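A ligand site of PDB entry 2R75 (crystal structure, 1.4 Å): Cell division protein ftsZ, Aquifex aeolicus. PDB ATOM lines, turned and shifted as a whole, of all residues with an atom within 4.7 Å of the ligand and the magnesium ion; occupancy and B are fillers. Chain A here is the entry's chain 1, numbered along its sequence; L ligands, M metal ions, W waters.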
ATOM      1  N   VAL A  15      -3.539  16.526  26.918  1.00  0.00           N
ATOM      2  CA  VAL A  15      -2.258  16.601  27.608  1.00  0.00           C
ATOM      3  C   VAL A  15      -2.081  17.996  28.149  1.00  0.00           C
ATOM      4  O   VAL A  15      -2.047  18.952  27.370  1.00  0.00           O
ATOM      5  CB  VAL A  15      -1.093  16.241  26.619  1.00  0.00           C
ATOM      6  CG1 VAL A  15       0.182  16.161  27.365  1.00  0.00           C
ATOM      7  CG2 VAL A  15      -1.381  14.956  25.857  1.00  0.00           C
ATOM      8  N   GLY A  16      -1.911  18.083  29.477  1.00  0.00           N
ATOM      9  CA  GLY A  16      -1.875  19.359  30.109  1.00  0.00           C
ATOM     10  C   GLY A  16      -3.243  19.973  30.305  1.00  0.00           C
ATOM     11  O   GLY A  16      -4.278  19.386  29.953  1.00  0.00           O
ATOM     12  N   GLY A  17      -3.263  21.198  30.821  1.00  0.00           N
ATOM     13  CA  GLY A  17      -4.550  21.836  31.227  1.00  0.00           C
ATOM     14  C   GLY A  17      -5.467  22.139  30.062  1.00  0.00           C
ATOM     15  O   GLY A  17      -6.626  21.761  30.045  1.00  0.00           O
ATOM     16  N   GLY A  18      -4.956  22.879  29.093  1.00  0.00           N
ATOM     17  CA  GLY A  18      -5.783  23.244  27.981  1.00  0.00           C
ATOM     18  C   GLY A  18      -6.234  22.075  27.137  1.00  0.00           C
ATOM     19  O   GLY A  18      -7.381  21.976  26.769  1.00  0.00           O
ATOM     20  N   GLY A  19      -5.307  21.152  26.865  1.00  0.00           N
ATOM     21  CA  GLY A  19      -5.639  19.955  26.149  1.00  0.00           C
ATOM     22  C   GLY A  19      -6.712  19.140  26.842  1.00  0.00           C
ATOM     23  O   GLY A  19      -7.610  18.570  26.207  1.00  0.00           O
ATOM     24  N   ASN A  21      -8.905  20.322  29.006  1.00  0.00           N
ATOM     25  CA  ASN A  21     -10.165  21.042  28.910  1.00  0.00           C
ATOM     26  C   ASN A  21     -10.878  20.795  27.576  1.00  0.00           C
ATOM     27  O   ASN A  21     -12.126  20.738  27.547  1.00  0.00           O
ATOM     28  CB  ASN A  21      -9.980  22.532  29.219  1.00  0.00           C
ATOM     29  CG  ASN A  21      -9.737  22.820  30.652  1.00  0.00           C
ATOM     30  OD1 ASN A  21      -9.892  21.952  31.480  1.00  0.00           O
ATOM     31  ND2 ASN A  21      -9.333  24.063  30.955  1.00  0.00           N
ATOM     32  N   ALA A  22     -10.123  20.690  26.485  1.00  0.00           N
ATOM     33  CA  ALA A  22     -10.789  20.401  25.197  1.00  0.00           C
ATOM     34  C   ALA A  22     -11.416  19.039  25.197  1.00  0.00           C
ATOM     35  O   ALA A  22     -12.515  18.840  24.649  1.00  0.00           O
ATOM     36  CB  ALA A  22      -9.754  20.564  24.042  1.00  0.00           C
ATOM     37  N   ASN A  40      -2.030  14.739  32.920  1.00  0.00           N
ATOM     38  CA  ASN A  40      -1.450  15.981  33.429  1.00  0.00           C
ATOM     39  C   ASN A  40      -0.450  15.709  34.507  1.00  0.00           C
ATOM     40  O   ASN A  40      -0.466  14.653  35.126  1.00  0.00           O
ATOM     41  CB  ASN A  40      -2.553  16.942  33.948  1.00  0.00           C
ATOM     42  CG  ASN A  40      -2.245  18.446  33.780  1.00  0.00           C
ATOM     43  OD1 ASN A  40      -1.132  18.868  33.685  1.00  0.00           O
ATOM     44  ND2 ASN A  40      -3.320  19.232  33.735  1.00  0.00           N
ATOM     45  N   THR A  41       0.417  16.694  34.706  1.00  0.00           N
ATOM     46  CA  THR A  41       1.341  16.711  35.829  1.00  0.00           C
ATOM     47  C   THR A  41       0.729  17.458  37.024  1.00  0.00           C
ATOM     48  O   THR A  41       1.257  17.393  38.106  1.00  0.00           O
ATOM     49  CB  THR A  41       2.606  17.507  35.447  1.00  0.00           C
ATOM     50  OG1 THR A  41       2.208  18.790  34.948  1.00  0.00           O
ATOM     51  CG2 THR A  41       3.473  16.778  34.403  1.00  0.00           C
ATOM     52  N   ASP A  42      -0.381  18.142  36.822  1.00  0.00           N
ATOM     53  CA  ASP A  42      -1.069  18.937  37.822  1.00  0.00           C
ATOM     54  C   ASP A  42      -2.313  18.125  38.288  1.00  0.00           C
ATOM     55  O   ASP A  42      -3.360  18.008  37.621  1.00  0.00           O
ATOM     56  CB  ASP A  42      -1.497  20.252  37.150  1.00  0.00           C
ATOM     57  CG  ASP A  42      -2.447  21.119  37.941  1.00  0.00           C
ATOM     58  OD1 ASP A  42      -2.916  20.779  39.065  1.00  0.00           O
ATOM     59  OD2 ASP A  42      -2.793  22.201  37.352  1.00  0.00           O
ATOM     60  N   GLY A  66       2.380  20.387  38.591  1.00  0.00           N
ATOM     61  CA  GLY A  66       2.540  20.969  37.268  1.00  0.00           C
ATOM     62  C   GLY A  66       3.995  21.166  36.904  1.00  0.00           C
ATOM     63  O   GLY A  66       4.881  20.974  37.716  1.00  0.00           O
ATOM     64  N   ALA A  67       4.230  21.582  35.644  1.00  0.00           N
ATOM     65  CA  ALA A  67       5.558  21.666  35.083  1.00  0.00           C
ATOM     66  C   ALA A  67       6.129  23.102  35.074  1.00  0.00           C
ATOM     67  O   ALA A  67       7.203  23.328  34.479  1.00  0.00           O
ATOM     68  CB  ALA A  67       5.615  21.071  33.703  1.00  0.00           C
ATOM     69  N   GLY A  68       5.404  24.057  35.627  1.00  0.00           N
ATOM     70  CA  GLY A  68       5.952  25.414  35.796  1.00  0.00           C
ATOM     71  C   GLY A  68       6.282  26.071  34.507  1.00  0.00           C
ATOM     72  O   GLY A  68       7.195  26.883  34.444  1.00  0.00           O
ATOM     73  N   ALA A  69       5.542  25.733  33.446  1.00  0.00           N
ATOM     74  CA  ALA A  69       5.716  26.349  32.124  1.00  0.00           C
ATOM     75  C   ALA A  69       7.025  25.948  31.468  1.00  0.00           C
ATOM     76  O   ALA A  69       7.436  26.554  30.467  1.00  0.00           O
ATOM     77  CB  ALA A  69       5.592  27.929  32.202  1.00  0.00           C
ATOM     78  N   LYS A  70       7.649  24.866  31.911  1.00  0.00           N
ATOM     79  CA  LYS A  70       8.916  24.420  31.347  1.00  0.00           C
ATOM     80  C   LYS A  70       8.703  23.148  30.522  1.00  0.00           C
ATOM     81  O   LYS A  70       8.501  22.074  31.088  1.00  0.00           O
ATOM     82  CB  LYS A  70       9.879  24.101  32.481  1.00  0.00           C
ATOM     83  CG  LYS A  70      10.199  25.289  33.407  1.00  0.00           C
ATOM     84  CD  LYS A  70      11.295  24.889  34.400  1.00  0.00           C
ATOM     85  CE  LYS A  70      12.669  25.094  33.777  1.00  0.00           C
ATOM     86  NZ  LYS A  70      13.747  24.324  34.489  1.00  0.00           N
ATOM     87  N   GLY A 100      -2.730  22.252  24.299  1.00  0.00           N
ATOM     88  CA  GLY A 100      -2.567  23.696  24.161  1.00  0.00           C
ATOM     89  C   GLY A 100      -1.088  23.956  24.241  1.00  0.00           C
ATOM     90  O   GLY A 100      -0.484  23.768  25.293  1.00  0.00           O
ATOM     91  N   LEU A 101      -0.445  24.358  23.147  1.00  0.00           N
ATOM     92  CA  LEU A 101       0.984  24.607  23.176  1.00  0.00           C
ATOM     93  C   LEU A 101       1.300  25.952  23.792  1.00  0.00           C
ATOM     94  O   LEU A 101       0.517  26.894  23.696  1.00  0.00           O
ATOM     95  CB  LEU A 101       1.633  24.468  21.775  1.00  0.00           C
ATOM     96  CG  LEU A 101       1.375  23.112  21.085  1.00  0.00           C
ATOM     97  CD1 LEU A 101       2.069  23.088  19.724  1.00  0.00           C
ATOM     98  CD2 LEU A 101       1.848  21.945  21.921  1.00  0.00           C
ATOM     99  N   GLY A 102       2.417  25.945  24.515  1.00  0.00           N
ATOM    100  CA  GLY A 102       2.877  27.178  25.190  1.00  0.00           C
ATOM    101  C   GLY A 102       3.134  27.008  26.669  1.00  0.00           C
ATOM    102  O   GLY A 102       3.823  27.856  27.255  1.00  0.00           O
ATOM    103  N   GLY A 103       2.600  25.961  27.310  1.00  0.00           N
ATOM    104  CA  GLY A 103       2.906  25.620  28.700  1.00  0.00           C
ATOM    105  C   GLY A 103       3.943  24.499  28.759  1.00  0.00           C
ATOM    106  O   GLY A 103       4.598  24.186  27.778  1.00  0.00           O
ATOM    107  N   GLY A 104       4.142  23.932  29.916  1.00  0.00           N
ATOM    108  CA  GLY A 104       5.167  22.915  30.064  1.00  0.00           C
ATOM    109  C   GLY A 104       4.715  21.523  29.727  1.00  0.00           C
ATOM    110  O   GLY A 104       5.441  20.737  29.138  1.00  0.00           O
ATOM    111  N   THR A 105       3.509  21.157  30.173  1.00  0.00           N
ATOM    112  CA  THR A 105       3.099  19.772  30.104  1.00  0.00           C
ATOM    113  C   THR A 105       2.639  19.399  28.694  1.00  0.00           C
ATOM    114  O   THR A 105       3.134  18.452  28.089  1.00  0.00           O
ATOM    115  CB  THR A 105       2.011  19.459  31.182  1.00  0.00           C
ATOM    116  OG1 THR A 105       2.575  19.684  32.460  1.00  0.00           O
ATOM    117  CG2 THR A 105       1.541  18.013  31.106  1.00  0.00           C
ATOM    118  N   GLY A 106       1.656  20.118  28.134  1.00  0.00           N
ATOM    119  CA  GLY A 106       1.259  19.862  26.750  1.00  0.00           C
ATOM    120  C   GLY A 106       2.470  19.979  25.816  1.00  0.00           C
ATOM    121  O   GLY A 106       2.747  19.054  25.041  1.00  0.00           O
ATOM    122  N   THR A 129      -3.108  23.728  19.715  1.00  0.00           N
ATOM    123  CA  THR A 129      -3.373  25.159  19.580  1.00  0.00           C
ATOM    124  C   THR A 129      -2.127  25.988  19.796  1.00  0.00           C
ATOM    125  O   THR A 129      -1.238  25.592  20.551  1.00  0.00           O
ATOM    126  CB  THR A 129      -4.495  25.644  20.536  1.00  0.00           C
ATOM    127  OG1 THR A 129      -4.106  25.479  21.893  1.00  0.00           O
ATOM    128  CG2 THR A 129      -5.816  24.958  20.232  1.00  0.00           C
ATOM    129  N   PRO A 131      -1.189  29.924  21.059  1.00  0.00           N
ATOM    130  CA  PRO A 131      -1.838  30.844  21.982  1.00  0.00           C
ATOM    131  C   PRO A 131      -2.395  32.122  21.416  1.00  0.00           C
ATOM    132  O   PRO A 131      -1.989  32.578  20.354  1.00  0.00           O
ATOM    133  CB  PRO A 131      -0.742  31.107  23.037  1.00  0.00           C
ATOM    134  CG  PRO A 131       0.541  30.737  22.381  1.00  0.00           C
ATOM    135  CD  PRO A 131       0.215  29.662  21.421  1.00  0.00           C
ATOM    136  N   GLU A 135      -1.748  36.314  25.428  1.00  0.00           N
ATOM    137  CA  GLU A 135      -0.846  35.461  26.229  1.00  0.00           C
ATOM    138  C   GLU A 135       0.605  35.814  26.118  1.00  0.00           C
ATOM    139  O   GLU A 135       1.420  35.298  26.825  1.00  0.00           O
ATOM    140  CB  GLU A 135      -1.050  34.005  25.834  1.00  0.00           C
ATOM    141  CG  GLU A 135      -2.468  33.550  26.080  1.00  0.00           C
ATOM    142  CD  GLU A 135      -2.600  32.057  25.883  1.00  0.00           C
ATOM    143  OE1 GLU A 135      -2.037  31.337  26.761  1.00  0.00           O
ATOM    144  OE2 GLU A 135      -3.302  31.599  24.925  1.00  0.00           O
ATOM    145  N   LYS A 139       5.046  32.760  25.399  1.00  0.00           N
ATOM    146  CA  LYS A 139       4.206  31.571  25.224  1.00  0.00           C
ATOM    147  C   LYS A 139       4.189  31.159  23.778  1.00  0.00           C
ATOM    148  O   LYS A 139       4.267  29.969  23.490  1.00  0.00           O
ATOM    149  CB  LYS A 139       2.817  31.787  25.792  1.00  0.00           C
ATOM    150  CG  LYS A 139       2.825  31.734  27.357  1.00  0.00           C
ATOM    151  CD  LYS A 139       1.476  31.336  27.864  1.00  0.00           C
ATOM    152  CE  LYS A 139       1.408  29.849  28.066  1.00  0.00           C
ATOM    153  NZ  LYS A 139       2.265  29.332  29.193  1.00  0.00           N
ATOM    154  N   ASN A 162      -5.320  30.293  18.101  1.00  0.00           N
ATOM    155  CA  ASN A 162      -6.475  30.781  18.852  1.00  0.00           C
ATOM    156  C   ASN A 162      -6.919  32.168  18.353  1.00  0.00           C
ATOM    157  O   ASN A 162      -8.103  32.476  18.422  1.00  0.00           O
ATOM    158  CB  ASN A 162      -6.150  30.841  20.331  1.00  0.00           C
ATOM    159  CG  ASN A 162      -6.043  29.492  20.973  1.00  0.00           C
ATOM    160  OD1 ASN A 162      -6.338  28.505  20.331  1.00  0.00           O
ATOM    161  ND2 ASN A 162      -5.659  29.459  22.243  1.00  0.00           N
ATOM    162  N   PHE A 179     -11.722  30.951  25.896  1.00  0.00           N
ATOM    163  CA  PHE A 179     -11.324  29.531  25.807  1.00  0.00           C
ATOM    164  C   PHE A 179     -12.444  28.570  25.602  1.00  0.00           C
ATOM    165  O   PHE A 179     -12.221  27.527  25.003  1.00  0.00           O
ATOM    166  CB  PHE A 179     -10.441  29.174  26.987  1.00  0.00           C
ATOM    167  CG  PHE A 179      -9.071  29.709  26.846  1.00  0.00           C
ATOM    168  CD1 PHE A 179      -8.187  29.173  25.905  1.00  0.00           C
ATOM    169  CD2 PHE A 179      -8.642  30.794  27.602  1.00  0.00           C
ATOM    170  CE1 PHE A 179      -6.961  29.665  25.790  1.00  0.00           C
ATOM    171  CE2 PHE A 179      -7.372  31.318  27.456  1.00  0.00           C
ATOM    172  CZ  PHE A 179      -6.523  30.734  26.558  1.00  0.00           C
ATOM    173  N   VAL A 182     -12.734  28.278  21.943  1.00  0.00           N
ATOM    174  CA  VAL A 182     -11.674  27.365  21.448  1.00  0.00           C
ATOM    175  C   VAL A 182     -12.061  25.925  21.678  1.00  0.00           C
ATOM    176  O   VAL A 182     -11.975  25.111  20.749  1.00  0.00           O
ATOM    177  CB  VAL A 182     -10.298  27.680  22.109  1.00  0.00           C
ATOM    178  CG1 VAL A 182      -9.232  26.700  21.698  1.00  0.00           C
ATOM    179  CG2 VAL A 182      -9.859  29.116  21.739  1.00  0.00           C
ATOM    180  N   ASP A 183     -12.496  25.585  22.890  1.00  0.00           N
ATOM    181  CA  ASP A 183     -12.853  24.203  23.198  1.00  0.00           C
ATOM    182  C   ASP A 183     -13.988  23.729  22.265  1.00  0.00           C
ATOM    183  O   ASP A 183     -14.009  22.604  21.830  1.00  0.00           O
ATOM    184  CB  ASP A 183     -13.420  24.001  24.636  1.00  0.00           C
ATOM    185  CG  ASP A 183     -12.479  24.234  25.823  1.00  0.00           C
ATOM    186  OD1 ASP A 183     -11.277  24.184  25.724  1.00  0.00           O
ATOM    187  OD2 ASP A 183     -13.042  24.381  26.969  1.00  0.00           O
ATOM    188  N   LEU A 186     -12.468  22.930  18.822  1.00  0.00           N
ATOM    189  CA  LEU A 186     -11.677  21.700  18.884  1.00  0.00           C
ATOM    190  C   LEU A 186     -12.573  20.481  18.984  1.00  0.00           C
ATOM    191  O   LEU A 186     -12.306  19.451  18.343  1.00  0.00           O
ATOM    192  CB  LEU A 186     -10.735  21.733  20.106  1.00  0.00           C
ATOM    193  CG  LEU A 186      -9.660  22.824  20.092  1.00  0.00           C
ATOM    194  CD1 LEU A 186      -8.957  22.912  21.425  1.00  0.00           C
ATOM    195  CD2 LEU A 186      -8.683  22.568  18.971  1.00  0.00           C
HETATM  196  C1  LIG L   1      -3.963  27.886  29.982  1.00  0.00           C
HETATM  197  C2  LIG L   1      -3.064  28.956  30.484  1.00  0.00           C
HETATM  198  O1  LIG L   1      -3.701  29.925  31.285  1.00  0.00           O
HETATM  199  C3  LIG L   1      -4.702  30.636  30.539  1.00  0.00           C
HETATM  200  C4  LIG L   1      -5.683  29.677  29.860  1.00  0.00           C
HETATM  201  N1  LIG L   1      -5.046  28.458  29.276  1.00  0.00           N
HETATM  202  C5  LIG L   1      -5.761  27.673  28.498  1.00  0.00           C
HETATM  203  N2  LIG L   1      -6.980  27.373  28.946  1.00  0.00           N
HETATM  204  C6  LIG L   1      -7.523  26.582  28.000  1.00  0.00           C
HETATM  205  C7  LIG L   1      -8.774  26.006  27.854  1.00  0.00           C
HETATM  206  O2  LIG L   1      -9.662  26.041  28.754  1.00  0.00           O
HETATM  207  N3  LIG L   1      -8.985  25.321  26.724  1.00  0.00           N
HETATM  208  C8  LIG L   1      -8.093  25.191  25.748  1.00  0.00           C
HETATM  209  N4  LIG L   1      -8.458  24.457  24.674  1.00  0.00           N
HETATM  210  N5  LIG L   1      -6.899  25.742  25.829  1.00  0.00           N
HETATM  211  C9  LIG L   1      -6.618  26.450  26.953  1.00  0.00           C
HETATM  212  N6  LIG L   1      -5.506  27.108  27.276  1.00  0.00           N
HETATM  213  C10 LIG L   1      -4.387  27.190  26.407  1.00  0.00           C
HETATM  214  O3  LIG L   1      -3.405  26.155  26.872  1.00  0.00           O
HETATM  215  C11 LIG L   1      -3.595  28.460  26.320  1.00  0.00           C
HETATM  216  O4  LIG L   1      -3.605  28.920  24.964  1.00  0.00           O
HETATM  217  C12 LIG L   1      -2.194  28.111  26.856  1.00  0.00           C
HETATM  218  O5  LIG L   1      -1.175  28.860  26.236  1.00  0.00           O
HETATM  219  C13 LIG L   1      -2.057  26.671  26.574  1.00  0.00           C
HETATM  220  C14 LIG L   1      -1.084  25.940  27.502  1.00  0.00           C
HETATM  221  O6  LIG L   1      -1.453  26.132  28.825  1.00  0.00           O
HETATM  222  P1  LIG L   1      -1.758  24.895  29.759  1.00  0.00           P
HETATM  223  O7  LIG L   1      -2.528  25.392  30.937  1.00  0.00           O
HETATM  224  O8  LIG L   1      -2.376  23.779  28.981  1.00  0.00           O
HETATM  225  O9  LIG L   1      -0.294  24.452  30.258  1.00  0.00           O
HETATM  226  P2  LIG L   1       0.127  22.981  30.670  1.00  0.00           P
HETATM  227  O10 LIG L   1      -0.814  22.468  31.706  1.00  0.00           O
HETATM  228  O11 LIG L   1       0.272  22.124  29.478  1.00  0.00           O
HETATM  229  O12 LIG L   1       1.547  23.228  31.295  1.00  0.00           O
HETATM  230  P3  LIG L   1       2.112  23.449  32.862  1.00  0.00           P
HETATM  231  O13 LIG L   1       0.864  24.100  33.564  1.00  0.00           O
HETATM  232  O14 LIG L   1       2.409  22.009  33.433  1.00  0.00           O
HETATM  233  O15 LIG L   1       3.300  24.300  32.631  1.00  0.00           O
HETATM  234 MG    MG M   1      -0.983  23.137  33.908  1.00  0.00          MG
HETATM  235  O   HOH W   1      -1.049  23.711  35.875  1.00  0.00           O
HETATM  236  O   HOH W   2      -1.909  24.834  33.358  1.00  0.00           O
HETATM  237  O   HOH W   3      -9.435  28.788  30.713  1.00  0.00           O
HETATM  238  O   HOH W   4      -2.360  27.327  22.954  1.00  0.00           O
HETATM  239  O   HOH W   5      -2.428  21.624  27.158  1.00  0.00           O
HETATM  240  O   HOH W   6     -12.210  25.965  28.959  1.00  0.00           O
HETATM  241  O   HOH W   7      -6.042  26.834  23.375  1.00  0.00           O
HETATM  242  O   HOH W   8      -5.907  23.764  23.418  1.00  0.00           O
HETATM  243  O   HOH W   9      -2.955  22.142  34.351  1.00  0.00           O
HETATM  244  O   HOH W  10       2.190  26.847  32.127  1.00  0.00           O
HETATM  245  O   HOH W  11      -5.051  25.214  32.127  1.00  0.00           O
HETATM  246  O   HOH W  12       0.421  27.992  30.252  1.00  0.00           O
HETATM  247  O   HOH W  13       1.419  23.224  27.099  1.00  0.00           O
HETATM  248  O   HOH W  14       0.009  21.317  34.354  1.00  0.00           O
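The side-chain hydroxyl (OG1) of Thr 41 lies within hydrogen-bond range of the side-chain hydroxyl (OG1) of Thr 105 (2.7 Å).
The side-chain amino group (NZ) of Lys 139 is in hydrogen-bond range of the backbone carbonyl oxygen (O) of Gly 102 (2.9 Å).
N of Gly 66 lies within hydrogen-bond range of O of Thr 41 (3.2 Å).
The backbone NH of Leu 101 lies within hydrogen-bond range of the backbone carbonyl oxygen of Thr 129 (3.0 Å).
No residue comes within 4 Å of the magnesium ion.
Residues that only touch the ligand: Gly 100 (3.2 Å), Phe 179 (3.3 Å), Lys 139 (3.3 Å), Gly 16 (3.6 Å), Thr 41 (3.6 Å), Leu 101 (3.6 Å), Leu 186 (3.6 Å), Gly 68 (3.7 Å), Gly 103 (3.7 Å), Val 182 (3.8 Å), Gly 66 (3.9 Å) and Pro 131 (3.9 Å).
Hydrophobic or aromatic side chains that line the ligand: Ala 67, Pro 131, Phe 179, Val 182 and Leu 186.
23 residues have an atom within 4 Å of the ligand: Gly 16, Gly 17, Gly 18, Asn 21, Thr 41, Gly 66, Ala 67, Gly 68, Ala 69, Gly 100, Leu 101, Gly 103, Gly 104, Thr 105, Gly 106, Pro 131, Glu 135, Lys 139, Asn 162, Phe 179, Val 182, Asp 183 and Leu 186.
The nearest printed residue that does not touch the ligand is Asn 40 (4.1 Å).
The backbone NH (N) of Thr 105 sits at hydrogen-bond distance from an oxygen (O12) of the ligand, at 3.1 Å.
The side-chain hydroxyl of Thr 105 lies within hydrogen-bond range of an oxygen (O14) of the ligand, 2.5 Å away.
The side-chain carboxylate of Glu 135 is in hydrogen-bond range of an oxygen (O5) of the ligand, at 2.7 Å.
N of Gly 18 is in hydrogen-bond range of O8 of the ligand, 2.7 Å away.
The backbone carbonyl oxygen (O) of Gly 18 lies within hydrogen-bond range of a nitrogen (N4) of the ligand.
The side-chain carboxylate (OD1) of Asp 183 is in hydrogen-bond range of a nitrogen (N3) of the ligand, 2.7 Å away.
O15 of the ligand lies within hydrogen-bond range of N of Ala 69.
An oxygen (O11) of the ligand lies within hydrogen-bond range of the backbone NH of Gly 106, 2.8 Å away.
The backbone NH (N) of Gly 104 is in hydrogen-bond range of an oxygen (O15) of the ligand, 2.9 Å away.
The backbone NH (N) of Ala 67 sits at hydrogen-bond distance from an oxygen (O14) of the ligand.
The backbone NH of Gly 17 sits at hydrogen-bond distance from an oxygen (O8) of the ligand (3.3 Å).
O2 of the ligand lies within hydrogen-bond range of ND2 of Asn 21, 3.0 Å away.
The side-chain amide nitrogen of Asn 162 is in hydrogen-bond range of an oxygen (O4) of the ligand, at 3.5 Å.
Water W9 bridges the side-chain amide nitrogen (ND2) of Asn 40 (3.0 Å) and the side-chain carboxylate (OD2) of Asp 42 (3.0 Å).
Water W14 lies within hydrogen-bond range of O14 of the ligand (2.7 Å), OD1 of Asn 40 (2.8 Å) and OG1 of Thr 41 (3.4 Å).
Water W6 lies within hydrogen-bond range of O2 of the ligand and OD2 of Asp 183.
Water W4 lies within hydrogen-bond range of the side-chain hydroxyl of Thr 129, an oxygen (O4) of the ligand and the backbone carbonyl oxygen of Leu 101.
Water W13 lies within hydrogen-bond range of the backbone carbonyl oxygen of Gly 100, an oxygen (O11) of the ligand, the backbone NH of Gly 103 and the backbone NH of Gly 106.
Water W8 lies within hydrogen-bond range of OG1 of Thr 129 (2.9 Å) and N4 of the ligand (2.9 Å).
The magnesium ion is bound by water W2 (2.0 Å).
Water W1 is bound to the magnesium ion (2.1 Å).
O13 of the ligand is bound to the magnesium ion, at 2.1 Å.
Water W14 is bound to the magnesium ion (2.1 Å).
Water W9 is bound to the magnesium ion, at 2.3 Å.
An oxygen (O10) of the ligand binds the magnesium ion (2.3 Å).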
